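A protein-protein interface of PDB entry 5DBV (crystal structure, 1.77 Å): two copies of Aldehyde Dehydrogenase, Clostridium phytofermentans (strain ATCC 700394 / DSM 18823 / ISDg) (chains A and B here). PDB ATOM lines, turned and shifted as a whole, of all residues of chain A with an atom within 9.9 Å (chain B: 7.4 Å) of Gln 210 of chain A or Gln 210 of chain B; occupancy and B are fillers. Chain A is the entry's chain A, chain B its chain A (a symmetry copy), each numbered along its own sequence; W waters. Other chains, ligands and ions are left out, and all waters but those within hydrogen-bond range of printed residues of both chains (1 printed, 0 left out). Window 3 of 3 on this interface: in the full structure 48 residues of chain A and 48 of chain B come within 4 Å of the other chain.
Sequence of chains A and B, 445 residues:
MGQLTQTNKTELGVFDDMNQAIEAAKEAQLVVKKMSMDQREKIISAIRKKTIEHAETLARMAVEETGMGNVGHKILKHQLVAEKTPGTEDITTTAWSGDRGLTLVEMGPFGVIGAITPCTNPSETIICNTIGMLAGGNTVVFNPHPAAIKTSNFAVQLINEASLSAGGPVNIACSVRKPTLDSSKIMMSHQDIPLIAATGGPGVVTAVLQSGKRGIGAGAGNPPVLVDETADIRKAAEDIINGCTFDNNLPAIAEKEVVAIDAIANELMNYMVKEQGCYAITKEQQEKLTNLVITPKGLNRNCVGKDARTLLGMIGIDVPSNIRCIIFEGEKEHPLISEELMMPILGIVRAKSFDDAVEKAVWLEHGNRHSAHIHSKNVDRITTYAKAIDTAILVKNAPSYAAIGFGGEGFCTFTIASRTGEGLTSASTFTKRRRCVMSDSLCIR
The side-chain hydroxyl of Thr 206 of chain B lies within hydrogen-bond range of the guanidinium group of Arg 419 of chain B (2.7 Å).
The side-chain hydroxyl of Thr 206 of chain A is in hydrogen-bond range of the guanidinium group of Arg 419 of chain A (2.7 Å).
O of Val 208 of chain B lies within hydrogen-bond range of OG of Ser 211 of chain B (2.6 Å).
OG of Ser 211 of chain A sits close to N of Lys 213 of chain A (3.3 Å).
O of Met 188 of chain B lies close to NZ of Lys 213 of chain B (3.3 Å).
The side-chain hydroxyl (OG) of Ser 211 of chain A is in hydrogen-bond range of the backbone carbonyl oxygen (O) of Val 208 of chain A.
Leu 209 of chain A touches Gln 210 of chain B, and with the chains exchanged Gln 210 of chain A touches Leu 209 of chain B.
Leu 209 of chain A touches Ser 211 of chain B, and with the chains exchanged Ser 211 of chain A touches Leu 209 of chain B.
Leu 209 of chain A touches Gly 212 of chain B, and with the chains exchanged Gly 212 of chain A touches Leu 209 of chain B.
Gly 212 of chain A touches Arg 419 of chain B, and with the chains exchanged Arg 419 of chain A touches Gly 212 of chain B.
Of the 12 pairs that touch across the chains among the printed residues, 12 have their exchanged pair printed and touching as well.
Water W1 bridges the backbone carbonyl oxygen of Arg 419 of chain B and the backbone NH of Arg 214 of chain A.
Of the printed residues of chain B, Gln 210 of chain A touches Leu 209 (3.7 Å) and Gln 210 (3.6 Å).
Of the printed residues of chain A, Gln 210 of chain B touches Leu 209 (3.7 Å) and Gln 210 (3.6 Å).
No residue of chain A comes within 4 Å of Ala 207 of chain B.
Ser 211 of chain B touches just one residue of chain A: Leu 209.
Of the printed residues of chain B, Gly 212 of chain A touches Leu 209 and Arg 419.
Of the printed residues of chain B, Leu 209 of chain A touches Leu 209 (3.1 Å), Gln 210 (3.7 Å), Ser 211 (3.6 Å), Gly 212 (2.9 Å) and Lys 213 (3.99 Å).
Val 205 of chain A touches none of the printed residues of chain B.
Thr 206 of chain A touches none of the printed residues of chain B.
Hydrophobic or aromatic side chains of chain A that line the printed part of chain B: Leu 209.
Printed residues of chain B that touch a printed residue of chain A: Leu 209, Gln 210, Ser 211, Gly 212, Lys 213 and Arg 419.
Hydrophobic or aromatic side chains of chain B within 4 Å of the printed part of chain A: Leu 209.
O of Leu 209 of chain A touches C of Gln 210 of chain B, 3.7 Å away.
O of Leu 209 of chain A touches N of Ser 211 of chain B, at 3.6 Å.
CD2 of Leu 209 of chain A touches O of Lys 213 of chain B, 3.99 Å away.
C of Gln 210 of chain A touches O of Leu 209 of chain B, at 3.7 Å.
CG of Gln 210 of chain A touches O of Gln 210 of chain B, at 3.6 Å.
O of Leu 209 of chain B touches N of Ser 211 of chain A, 3.6 Å away.
Lys 213 of chain A touches Leu 209 of chain B (O to CD2, 3.99 Å).
NH1 of Arg 419 of chain A is in hydrogen-bond range of O of Gly 212 of chain B, 3.2 Å away.
The backbone carbonyl oxygen of Leu 209 of chain A sits close to the backbone carbonyl oxygen of Leu 209 of chain B, 3.1 Å away.
The guanidinium group (NH1) of Arg 419 of chain B sits at hydrogen-bond distance from the backbone carbonyl oxygen (O) of Gly 212 of chain A.
The backbone NH of Gly 212 of chain B is in hydrogen-bond range of the backbone carbonyl oxygen of Leu 209 of chain A (2.9 Å).
The backbone NH (N) of Gly 212 of chain A lies within hydrogen-bond range of the backbone carbonyl oxygen (O) of Leu 209 of chain B (2.9 Å).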
ATOM      1  N   LYS A 185      -7.137  33.275   6.583  1.00  0.00           N
ATOM      2  CA  LYS A 185      -6.016  32.397   6.261  1.00  0.00           C
ATOM      3  C   LYS A 185      -5.854  31.281   7.304  1.00  0.00           C
ATOM      4  O   LYS A 185      -5.509  30.158   6.960  1.00  0.00           O
ATOM      5  CB  LYS A 185      -4.727  33.205   6.116  1.00  0.00           C
ATOM      6  CG  LYS A 185      -4.686  34.029   4.829  1.00  0.00           C
ATOM      7  CD  LYS A 185      -3.409  34.873   4.735  1.00  0.00           C
ATOM      8  CE  LYS A 185      -3.246  35.525   3.363  1.00  0.00           C
ATOM      9  NZ  LYS A 185      -1.851  36.000   3.127  1.00  0.00           N
ATOM     10  N   MET A 188      -8.372  28.769   6.164  1.00  0.00           N
ATOM     11  CA  MET A 188      -7.999  28.120   4.908  1.00  0.00           C
ATOM     12  C   MET A 188      -6.923  27.084   5.096  1.00  0.00           C
ATOM     13  O   MET A 188      -6.837  26.149   4.316  1.00  0.00           O
ATOM     14  CB  MET A 188      -7.525  29.153   3.878  1.00  0.00           C
ATOM     15  CG  MET A 188      -8.670  29.844   3.158  1.00  0.00           C
ATOM     16  SD  MET A 188      -8.144  30.923   1.821  1.00  0.00           S
ATOM     17  CE  MET A 188      -7.295  32.211   2.731  1.00  0.00           C
ATOM     18  N   SER A 189      -6.089  27.248   6.116  1.00  0.00           N
ATOM     19  CA  SER A 189      -4.949  26.340   6.303  1.00  0.00           C
ATOM     20  C   SER A 189      -5.197  25.389   7.492  1.00  0.00           C
ATOM     21  O   SER A 189      -4.329  24.600   7.857  1.00  0.00           O
ATOM     22  CB  SER A 189      -3.656  27.136   6.501  1.00  0.00           C
ATOM     23  OG  SER A 189      -3.623  27.741   7.773  1.00  0.00           O
ATOM     24  N   GLN A 191      -6.275  22.274   9.511  1.00  0.00           N
ATOM     25  CA  GLN A 191      -6.388  20.892   9.091  1.00  0.00           C
ATOM     26  C   GLN A 191      -7.679  20.218   9.540  1.00  0.00           C
ATOM     27  O   GLN A 191      -7.944  19.088   9.158  1.00  0.00           O
ATOM     28  CB  GLN A 191      -5.174  20.123   9.592  1.00  0.00           C
ATOM     29  CG  GLN A 191      -3.874  20.658   8.991  1.00  0.00           C
ATOM     30  CD  GLN A 191      -3.900  20.640   7.472  1.00  0.00           C
ATOM     31  OE1 GLN A 191      -3.770  19.582   6.860  1.00  0.00           O
ATOM     32  NE2 GLN A 191      -4.106  21.806   6.856  1.00  0.00           N
ATOM     33  N   ILE A 196     -14.233  24.321   2.104  1.00  0.00           N
ATOM     34  CA  ILE A 196     -14.558  25.724   2.287  1.00  0.00           C
ATOM     35  C   ILE A 196     -15.537  26.128   1.218  1.00  0.00           C
ATOM     36  O   ILE A 196     -15.307  25.875   0.042  1.00  0.00           O
ATOM     37  CB  ILE A 196     -13.333  26.609   2.216  1.00  0.00           C
ATOM     38  CG1 ILE A 196     -12.450  26.332   3.430  1.00  0.00           C
ATOM     39  CG2 ILE A 196     -13.720  28.097   2.212  1.00  0.00           C
ATOM     40  CD1 ILE A 196     -11.067  26.817   3.284  1.00  0.00           C
ATOM     41  N   ALA A 198     -16.924  29.308  -0.566  1.00  0.00           N
ATOM     42  CA  ALA A 198     -16.454  30.659  -0.749  1.00  0.00           C
ATOM     43  C   ALA A 198     -17.458  31.437  -1.577  1.00  0.00           C
ATOM     44  O   ALA A 198     -17.570  31.232  -2.783  1.00  0.00           O
ATOM     45  CB  ALA A 198     -15.081  30.654  -1.413  1.00  0.00           C
ATOM     46  N   PRO A 202     -13.424  36.934  -7.056  1.00  0.00           N
ATOM     47  CA  PRO A 202     -12.303  36.106  -7.526  1.00  0.00           C
ATOM     48  C   PRO A 202     -11.122  36.086  -6.568  1.00  0.00           C
ATOM     49  O   PRO A 202     -10.355  35.122  -6.572  1.00  0.00           O
ATOM     50  CB  PRO A 202     -11.911  36.770  -8.850  1.00  0.00           C
ATOM     51  CG  PRO A 202     -13.170  37.372  -9.338  1.00  0.00           C
ATOM     52  CD  PRO A 202     -13.916  37.831  -8.117  1.00  0.00           C
ATOM     53  N   GLY A 203     -10.990  37.137  -5.760  1.00  0.00           N
ATOM     54  CA  GLY A 203      -9.895  37.244  -4.818  1.00  0.00           C
ATOM     55  C   GLY A 203      -9.943  36.135  -3.792  1.00  0.00           C
ATOM     56  O   GLY A 203      -9.053  35.289  -3.735  1.00  0.00           O
ATOM     57  N   VAL A 204     -10.993  36.130  -2.984  1.00  0.00           N
ATOM     58  CA  VAL A 204     -11.150  35.117  -1.947  1.00  0.00           C
ATOM     59  C   VAL A 204     -11.232  33.695  -2.525  1.00  0.00           C
ATOM     60  O   VAL A 204     -10.654  32.763  -1.976  1.00  0.00           O
ATOM     61  CB  VAL A 204     -12.404  35.396  -1.087  1.00  0.00           C
ATOM     62  CG1 VAL A 204     -12.181  36.620  -0.218  1.00  0.00           C
ATOM     63  CG2 VAL A 204     -13.639  35.590  -1.952  1.00  0.00           C
ATOM     64  N   VAL A 205     -11.915  33.542  -3.651  1.00  0.00           N
ATOM     65  CA  VAL A 205     -12.178  32.225  -4.225  1.00  0.00           C
ATOM     66  C   VAL A 205     -10.913  31.575  -4.754  1.00  0.00           C
ATOM     67  O   VAL A 205     -10.688  30.376  -4.569  1.00  0.00           O
ATOM     68  CB  VAL A 205     -13.215  32.327  -5.352  1.00  0.00           C
ATOM     69  CG1 VAL A 205     -13.510  30.957  -5.975  1.00  0.00           C
ATOM     70  CG2 VAL A 205     -14.483  32.939  -4.806  1.00  0.00           C
ATOM     71  N   THR A 206     -10.076  32.347  -5.432  1.00  0.00           N
ATOM     72  CA  THR A 206      -8.836  31.769  -5.917  1.00  0.00           C
ATOM     73  C   THR A 206      -7.985  31.327  -4.722  1.00  0.00           C
ATOM     74  O   THR A 206      -7.364  30.260  -4.754  1.00  0.00           O
ATOM     75  CB  THR A 206      -8.067  32.747  -6.802  1.00  0.00           C
ATOM     76  OG1 THR A 206      -8.879  33.057  -7.936  1.00  0.00           O
ATOM     77  CG2 THR A 206      -6.751  32.135  -7.273  1.00  0.00           C
ATOM     78  N   ALA A 207      -7.977  32.137  -3.664  1.00  0.00           N
ATOM     79  CA  ALA A 207      -7.195  31.803  -2.476  1.00  0.00           C
ATOM     80  C   ALA A 207      -7.685  30.480  -1.904  1.00  0.00           C
ATOM     81  O   ALA A 207      -6.900  29.636  -1.483  1.00  0.00           O
ATOM     82  CB  ALA A 207      -7.306  32.898  -1.434  1.00  0.00           C
ATOM     83  N   VAL A 208      -9.000  30.308  -1.908  1.00  0.00           N
ATOM     84  CA  VAL A 208      -9.581  29.082  -1.397  1.00  0.00           C
ATOM     85  C   VAL A 208      -9.197  27.919  -2.281  1.00  0.00           C
ATOM     86  O   VAL A 208      -8.877  26.857  -1.772  1.00  0.00           O
ATOM     87  CB  VAL A 208     -11.104  29.176  -1.288  1.00  0.00           C
ATOM     88  CG1 VAL A 208     -11.724  27.796  -1.009  1.00  0.00           C
ATOM     89  CG2 VAL A 208     -11.476  30.151  -0.190  1.00  0.00           C
ATOM     90  N   LEU A 209      -9.203  28.116  -3.598  1.00  0.00           N
ATOM     91  CA  LEU A 209      -8.808  27.046  -4.520  1.00  0.00           C
ATOM     92  C   LEU A 209      -7.313  26.825  -4.593  1.00  0.00           C
ATOM     93  O   LEU A 209      -6.847  25.965  -5.355  1.00  0.00           O
ATOM     94  CB  LEU A 209      -9.341  27.337  -5.914  1.00  0.00           C
ATOM     95  CG  LEU A 209     -10.866  27.274  -5.978  1.00  0.00           C
ATOM     96  CD1 LEU A 209     -11.357  27.871  -7.290  1.00  0.00           C
ATOM     97  CD2 LEU A 209     -11.366  25.825  -5.792  1.00  0.00           C
ATOM     98  N   GLN A 210      -6.562  27.601  -3.815  1.00  0.00           N
ATOM     99  CA  GLN A 210      -5.129  27.377  -3.639  1.00  0.00           C
ATOM    100  C   GLN A 210      -4.823  26.820  -2.260  1.00  0.00           C
ATOM    101  O   GLN A 210      -3.667  26.689  -1.879  1.00  0.00           O
ATOM    102  CB  GLN A 210      -4.342  28.671  -3.835  1.00  0.00           C
ATOM    103  CG  GLN A 210      -4.384  29.221  -5.240  1.00  0.00           C
ATOM    104  CD  GLN A 210      -3.825  30.628  -5.319  1.00  0.00           C
ATOM    105  OE1 GLN A 210      -3.532  31.246  -4.296  1.00  0.00           O
ATOM    106  NE2 GLN A 210      -3.674  31.140  -6.532  1.00  0.00           N
ATOM    107  N   SER A 211      -5.853  26.466  -1.504  1.00  0.00           N
ATOM    108  CA  SER A 211      -5.646  26.106  -0.089  1.00  0.00           C
ATOM    109  C   SER A 211      -5.292  24.639   0.199  1.00  0.00           C
ATOM    110  O   SER A 211      -4.979  24.290   1.340  1.00  0.00           O
ATOM    111  CB  SER A 211      -6.907  26.451   0.703  1.00  0.00           C
ATOM    112  OG  SER A 211      -7.953  25.580   0.336  1.00  0.00           O
ATOM    113  N   GLY A 212      -5.354  23.773  -0.805  1.00  0.00           N
ATOM    114  CA  GLY A 212      -5.130  22.357  -0.560  1.00  0.00           C
ATOM    115  C   GLY A 212      -6.351  21.647   0.001  1.00  0.00           C
ATOM    116  O   GLY A 212      -6.283  20.477   0.356  1.00  0.00           O
ATOM    117  N   LYS A 213      -7.467  22.372   0.069  1.00  0.00           N
ATOM    118  CA  LYS A 213      -8.768  21.860   0.486  1.00  0.00           C
ATOM    119  C   LYS A 213      -9.680  21.871  -0.722  1.00  0.00           C
ATOM    120  O   LYS A 213      -9.498  22.676  -1.639  1.00  0.00           O
ATOM    121  CB  LYS A 213      -9.426  22.737   1.579  1.00  0.00           C
ATOM    122  CG  LYS A 213      -8.711  22.806   2.897  1.00  0.00           C
ATOM    123  CD  LYS A 213      -9.376  23.824   3.832  1.00  0.00           C
ATOM    124  CE  LYS A 213      -8.633  23.918   5.184  1.00  0.00           C
ATOM    125  NZ  LYS A 213      -7.497  23.001   5.207  1.00  0.00           N
ATOM    126  N   ARG A 214     -10.702  21.039  -0.721  1.00  0.00           N
ATOM    127  CA  ARG A 214     -11.776  21.314  -1.653  1.00  0.00           C
ATOM    128  C   ARG A 214     -12.458  22.664  -1.381  1.00  0.00           C
ATOM    129  O   ARG A 214     -12.869  22.961  -0.245  1.00  0.00           O
ATOM    130  CB  ARG A 214     -12.830  20.251  -1.616  1.00  0.00           C
ATOM    131  CG  ARG A 214     -13.909  20.589  -2.619  1.00  0.00           C
ATOM    132  CD  ARG A 214     -14.780  19.424  -2.945  1.00  0.00           C
ATOM    133  NE  ARG A 214     -15.915  19.781  -3.809  1.00  0.00           N
ATOM    134  CZ  ARG A 214     -17.019  19.051  -3.864  1.00  0.00           C
ATOM    135  NH1 ARG A 214     -17.113  17.954  -3.109  1.00  0.00           N
ATOM    136  NH2 ARG A 214     -18.030  19.436  -4.621  1.00  0.00           N
ATOM    137  N   GLY A 215     -12.629  23.443  -2.439  1.00  0.00           N
ATOM    138  CA  GLY A 215     -13.319  24.722  -2.343  1.00  0.00           C
ATOM    139  C   GLY A 215     -14.518  24.730  -3.254  1.00  0.00           C
ATOM    140  O   GLY A 215     -14.418  24.359  -4.411  1.00  0.00           O
ATOM    141  N   ILE A 216     -15.667  25.147  -2.725  1.00  0.00           N
ATOM    142  CA  ILE A 216     -16.844  25.354  -3.534  1.00  0.00           C
ATOM    143  C   ILE A 216     -16.880  26.862  -3.724  1.00  0.00           C
ATOM    144  O   ILE A 216     -16.973  27.603  -2.749  1.00  0.00           O
ATOM    145  CB  ILE A 216     -18.065  24.789  -2.853  1.00  0.00           C
ATOM    146  CG1 ILE A 216     -17.910  23.258  -2.815  1.00  0.00           C
ATOM    147  CG2 ILE A 216     -19.374  25.254  -3.544  1.00  0.00           C
ATOM    148  CD1 ILE A 216     -18.837  22.586  -1.915  1.00  0.00           C
ATOM    149  N   ARG A 419     -17.954  29.007 -10.408  1.00  0.00           N
ATOM    150  CA  ARG A 419     -16.552  28.756 -10.721  1.00  0.00           C
ATOM    151  C   ARG A 419     -16.199  27.256 -10.666  1.00  0.00           C
ATOM    152  O   ARG A 419     -15.397  26.791 -11.493  1.00  0.00           O
ATOM    153  CB  ARG A 419     -15.657  29.527  -9.777  1.00  0.00           C
ATOM    154  CG  ARG A 419     -14.205  29.316 -10.070  1.00  0.00           C
ATOM    155  CD  ARG A 419     -13.425  30.596  -9.816  1.00  0.00           C
ATOM    156  NE  ARG A 419     -11.993  30.342  -9.753  1.00  0.00           N
ATOM    157  CZ  ARG A 419     -11.121  31.130  -9.135  1.00  0.00           C
ATOM    158  NH1 ARG A 419      -9.835  30.800  -9.126  1.00  0.00           N
ATOM    159  NH2 ARG A 419     -11.533  32.237  -8.521  1.00  0.00           N
ATOM    160  N   THR A 420     -16.776  26.514  -9.716  1.00  0.00           N
ATOM    161  CA  THR A 420     -16.357  25.136  -9.472  1.00  0.00           C
ATOM    162  C   THR A 420     -17.392  24.126  -9.966  1.00  0.00           C
ATOM    163  O   THR A 420     -17.106  22.926 -10.053  1.00  0.00           O
ATOM    164  CB  THR A 420     -16.013  24.906  -7.970  1.00  0.00           C
ATOM    165  OG1 THR A 420     -17.056  25.380  -7.130  1.00  0.00           O
ATOM    166  CG2 THR A 420     -14.712  25.621  -7.626  1.00  0.00           C
ATOM    167  N   MET B 188      -1.634  22.123 -14.750  1.00  0.00           N
ATOM    168  CA  MET B 188      -2.257  22.641 -13.533  1.00  0.00           C
ATOM    169  C   MET B 188      -2.469  24.131 -13.587  1.00  0.00           C
ATOM    170  O   MET B 188      -3.365  24.641 -12.932  1.00  0.00           O
ATOM    171  CB  MET B 188      -1.414  22.299 -12.299  1.00  0.00           C
ATOM    172  CG  MET B 188      -1.646  20.886 -11.792  1.00  0.00           C
ATOM    173  SD  MET B 188      -0.811  20.520 -10.244  1.00  0.00           S
ATOM    174  CE  MET B 188       0.905  20.578 -10.755  1.00  0.00           C
ATOM    175  N   GLY B 203       0.859  13.690  -2.846  1.00  0.00           N
ATOM    176  CA  GLY B 203       1.760  14.630  -3.477  1.00  0.00           C
ATOM    177  C   GLY B 203       1.085  15.360  -4.615  1.00  0.00           C
ATOM    178  O   GLY B 203       0.895  16.573  -4.564  1.00  0.00           O
ATOM    179  N   VAL B 204       0.708  14.616  -5.646  1.00  0.00           N
ATOM    180  CA  VAL B 204       0.053  15.204  -6.808  1.00  0.00           C
ATOM    181  C   VAL B 204      -1.277  15.884  -6.450  1.00  0.00           C
ATOM    182  O   VAL B 204      -1.587  16.957  -6.958  1.00  0.00           O
ATOM    183  CB  VAL B 204      -0.191  14.138  -7.902  1.00  0.00           C
ATOM    184  CG1 VAL B 204       1.125  13.722  -8.531  1.00  0.00           C
ATOM    185  CG2 VAL B 204      -0.908  12.920  -7.340  1.00  0.00           C
ATOM    186  N   VAL B 205      -2.038  15.279  -5.548  1.00  0.00           N
ATOM    187  CA  VAL B 205      -3.381  15.754  -5.224  1.00  0.00           C
ATOM    188  C   VAL B 205      -3.351  17.084  -4.494  1.00  0.00           C
ATOM    189  O   VAL B 205      -4.153  17.980  -4.769  1.00  0.00           O
ATOM    190  CB  VAL B 205      -4.128  14.716  -4.374  1.00  0.00           C
ATOM    191  CG1 VAL B 205      -5.542  15.190  -4.018  1.00  0.00           C
ATOM    192  CG2 VAL B 205      -4.186  13.409  -5.127  1.00  0.00           C
ATOM    193  N   THR B 206      -2.438  17.230  -3.544  1.00  0.00           N
ATOM    194  CA  THR B 206      -2.352  18.503  -2.853  1.00  0.00           C
ATOM    195  C   THR B 206      -1.965  19.595  -3.855  1.00  0.00           C
ATOM    196  O   THR B 206      -2.499  20.707  -3.809  1.00  0.00           O
ATOM    197  CB  THR B 206      -1.359  18.449  -1.694  1.00  0.00           C
ATOM    198  OG1 THR B 206      -1.818  17.473  -0.758  1.00  0.00           O
ATOM    199  CG2 THR B 206      -1.257  19.806  -1.002  1.00  0.00           C
ATOM    200  N   ALA B 207      -1.053  19.267  -4.770  1.00  0.00           N
ATOM    201  CA  ALA B 207      -0.617  20.240  -5.769  1.00  0.00           C
ATOM    202  C   ALA B 207      -1.812  20.679  -6.603  1.00  0.00           C
ATOM    203  O   ALA B 207      -1.970  21.853  -6.926  1.00  0.00           O
ATOM    204  CB  ALA B 207       0.457  19.650  -6.661  1.00  0.00           C
ATOM    205  N   VAL B 208      -2.661  19.716  -6.936  1.00  0.00           N
ATOM    206  CA  VAL B 208      -3.843  20.018  -7.721  1.00  0.00           C
ATOM    207  C   VAL B 208      -4.786  20.887  -6.923  1.00  0.00           C
ATOM    208  O   VAL B 208      -5.349  21.821  -7.470  1.00  0.00           O
ATOM    209  CB  VAL B 208      -4.562  18.747  -8.178  1.00  0.00           C
ATOM    210  CG1 VAL B 208      -5.943  19.077  -8.768  1.00  0.00           C
ATOM    211  CG2 VAL B 208      -3.712  18.023  -9.201  1.00  0.00           C
ATOM    212  N   LEU B 209      -4.944  20.603  -5.632  1.00  0.00           N
ATOM    213  CA  LEU B 209      -5.817  21.423  -4.784  1.00  0.00           C
ATOM    214  C   LEU B 209      -5.207  22.749  -4.384  1.00  0.00           C
ATOM    215  O   LEU B 209      -5.832  23.525  -3.647  1.00  0.00           O
ATOM    216  CB  LEU B 209      -6.202  20.650  -3.533  1.00  0.00           C
ATOM    217  CG  LEU B 209      -7.091  19.447  -3.844  1.00  0.00           C
ATOM    218  CD1 LEU B 209      -7.188  18.541  -2.624  1.00  0.00           C
ATOM    219  CD2 LEU B 209      -8.486  19.901  -4.325  1.00  0.00           C
ATOM    220  N   GLN B 210      -3.989  23.005  -4.856  1.00  0.00           N
ATOM    221  CA  GLN B 210      -3.355  24.314  -4.711  1.00  0.00           C
ATOM    222  C   GLN B 210      -3.310  25.055  -6.035  1.00  0.00           C
ATOM    223  O   GLN B 210      -2.702  26.112  -6.142  1.00  0.00           O
ATOM    224  CB  GLN B 210      -1.933  24.179  -4.171  1.00  0.00           C
ATOM    225  CG  GLN B 210      -1.848  23.651  -2.759  1.00  0.00           C
ATOM    226  CD  GLN B 210      -0.429  23.282  -2.373  1.00  0.00           C
ATOM    227  OE1 GLN B 210       0.473  23.291  -3.211  1.00  0.00           O
ATOM    228  NE2 GLN B 210      -0.224  22.956  -1.105  1.00  0.00           N
ATOM    229  N   SER B 211      -3.971  24.523  -7.054  1.00  0.00           N
ATOM    230  CA  SER B 211      -3.811  25.074  -8.411  1.00  0.00           C
ATOM    231  C   SER B 211      -4.736  26.242  -8.788  1.00  0.00           C
ATOM    232  O   SER B 211      -4.576  26.839  -9.856  1.00  0.00           O
ATOM    233  CB  SER B 211      -4.022  23.957  -9.432  1.00  0.00           C
ATOM    234  OG  SER B 211      -5.378  23.568  -9.439  1.00  0.00           O
ATOM    235  N   GLY B 212      -5.709  26.565  -7.946  1.00  0.00           N
ATOM    236  CA  GLY B 212      -6.673  27.593  -8.305  1.00  0.00           C
ATOM    237  C   GLY B 212      -7.771  27.086  -9.227  1.00  0.00           C
ATOM    238  O   GLY B 212      -8.594  27.860  -9.700  1.00  0.00           O
ATOM    239  N   LYS B 213      -7.770  25.776  -9.468  1.00  0.00           N
ATOM    240  CA  LYS B 213      -8.785  25.073 -10.245  1.00  0.00           C
ATOM    241  C   LYS B 213      -9.557  24.178  -9.299  1.00  0.00           C
ATOM    242  O   LYS B 213      -9.028  23.746  -8.272  1.00  0.00           O
ATOM    243  CB  LYS B 213      -8.170  24.174 -11.346  1.00  0.00           C
ATOM    244  CG  LYS B 213      -7.414  24.876 -12.435  1.00  0.00           C
ATOM    245  CD  LYS B 213      -6.727  23.870 -13.366  1.00  0.00           C
ATOM    246  CE  LYS B 213      -5.927  24.585 -14.478  1.00  0.00           C
ATOM    247  NZ  LYS B 213      -6.049  26.034 -14.343  1.00  0.00           N
ATOM    248  N   ARG B 419     -10.573  12.168  -1.057  1.00  0.00           N
ATOM    249  CA  ARG B 419     -10.095  13.406  -0.452  1.00  0.00           C
ATOM    250  C   ARG B 419     -11.102  14.562  -0.609  1.00  0.00           C
ATOM    251  O   ARG B 419     -11.243  15.374   0.321  1.00  0.00           O
ATOM    252  CB  ARG B 419      -8.764  13.802  -1.050  1.00  0.00           C
ATOM    253  CG  ARG B 419      -8.222  15.060  -0.447  1.00  0.00           C
ATOM    254  CD  ARG B 419      -6.706  14.984  -0.345  1.00  0.00           C
ATOM    255  NE  ARG B 419      -6.124  16.295  -0.094  1.00  0.00           N
ATOM    256  CZ  ARG B 419      -4.870  16.622  -0.382  1.00  0.00           C
ATOM    257  NH1 ARG B 419      -4.441  17.852  -0.124  1.00  0.00           N
ATOM    258  NH2 ARG B 419      -4.052  15.728  -0.933  1.00  0.00           N
HETATM  259  O   HOH W   1     -10.872  18.344   0.812  1.00  0.00           O
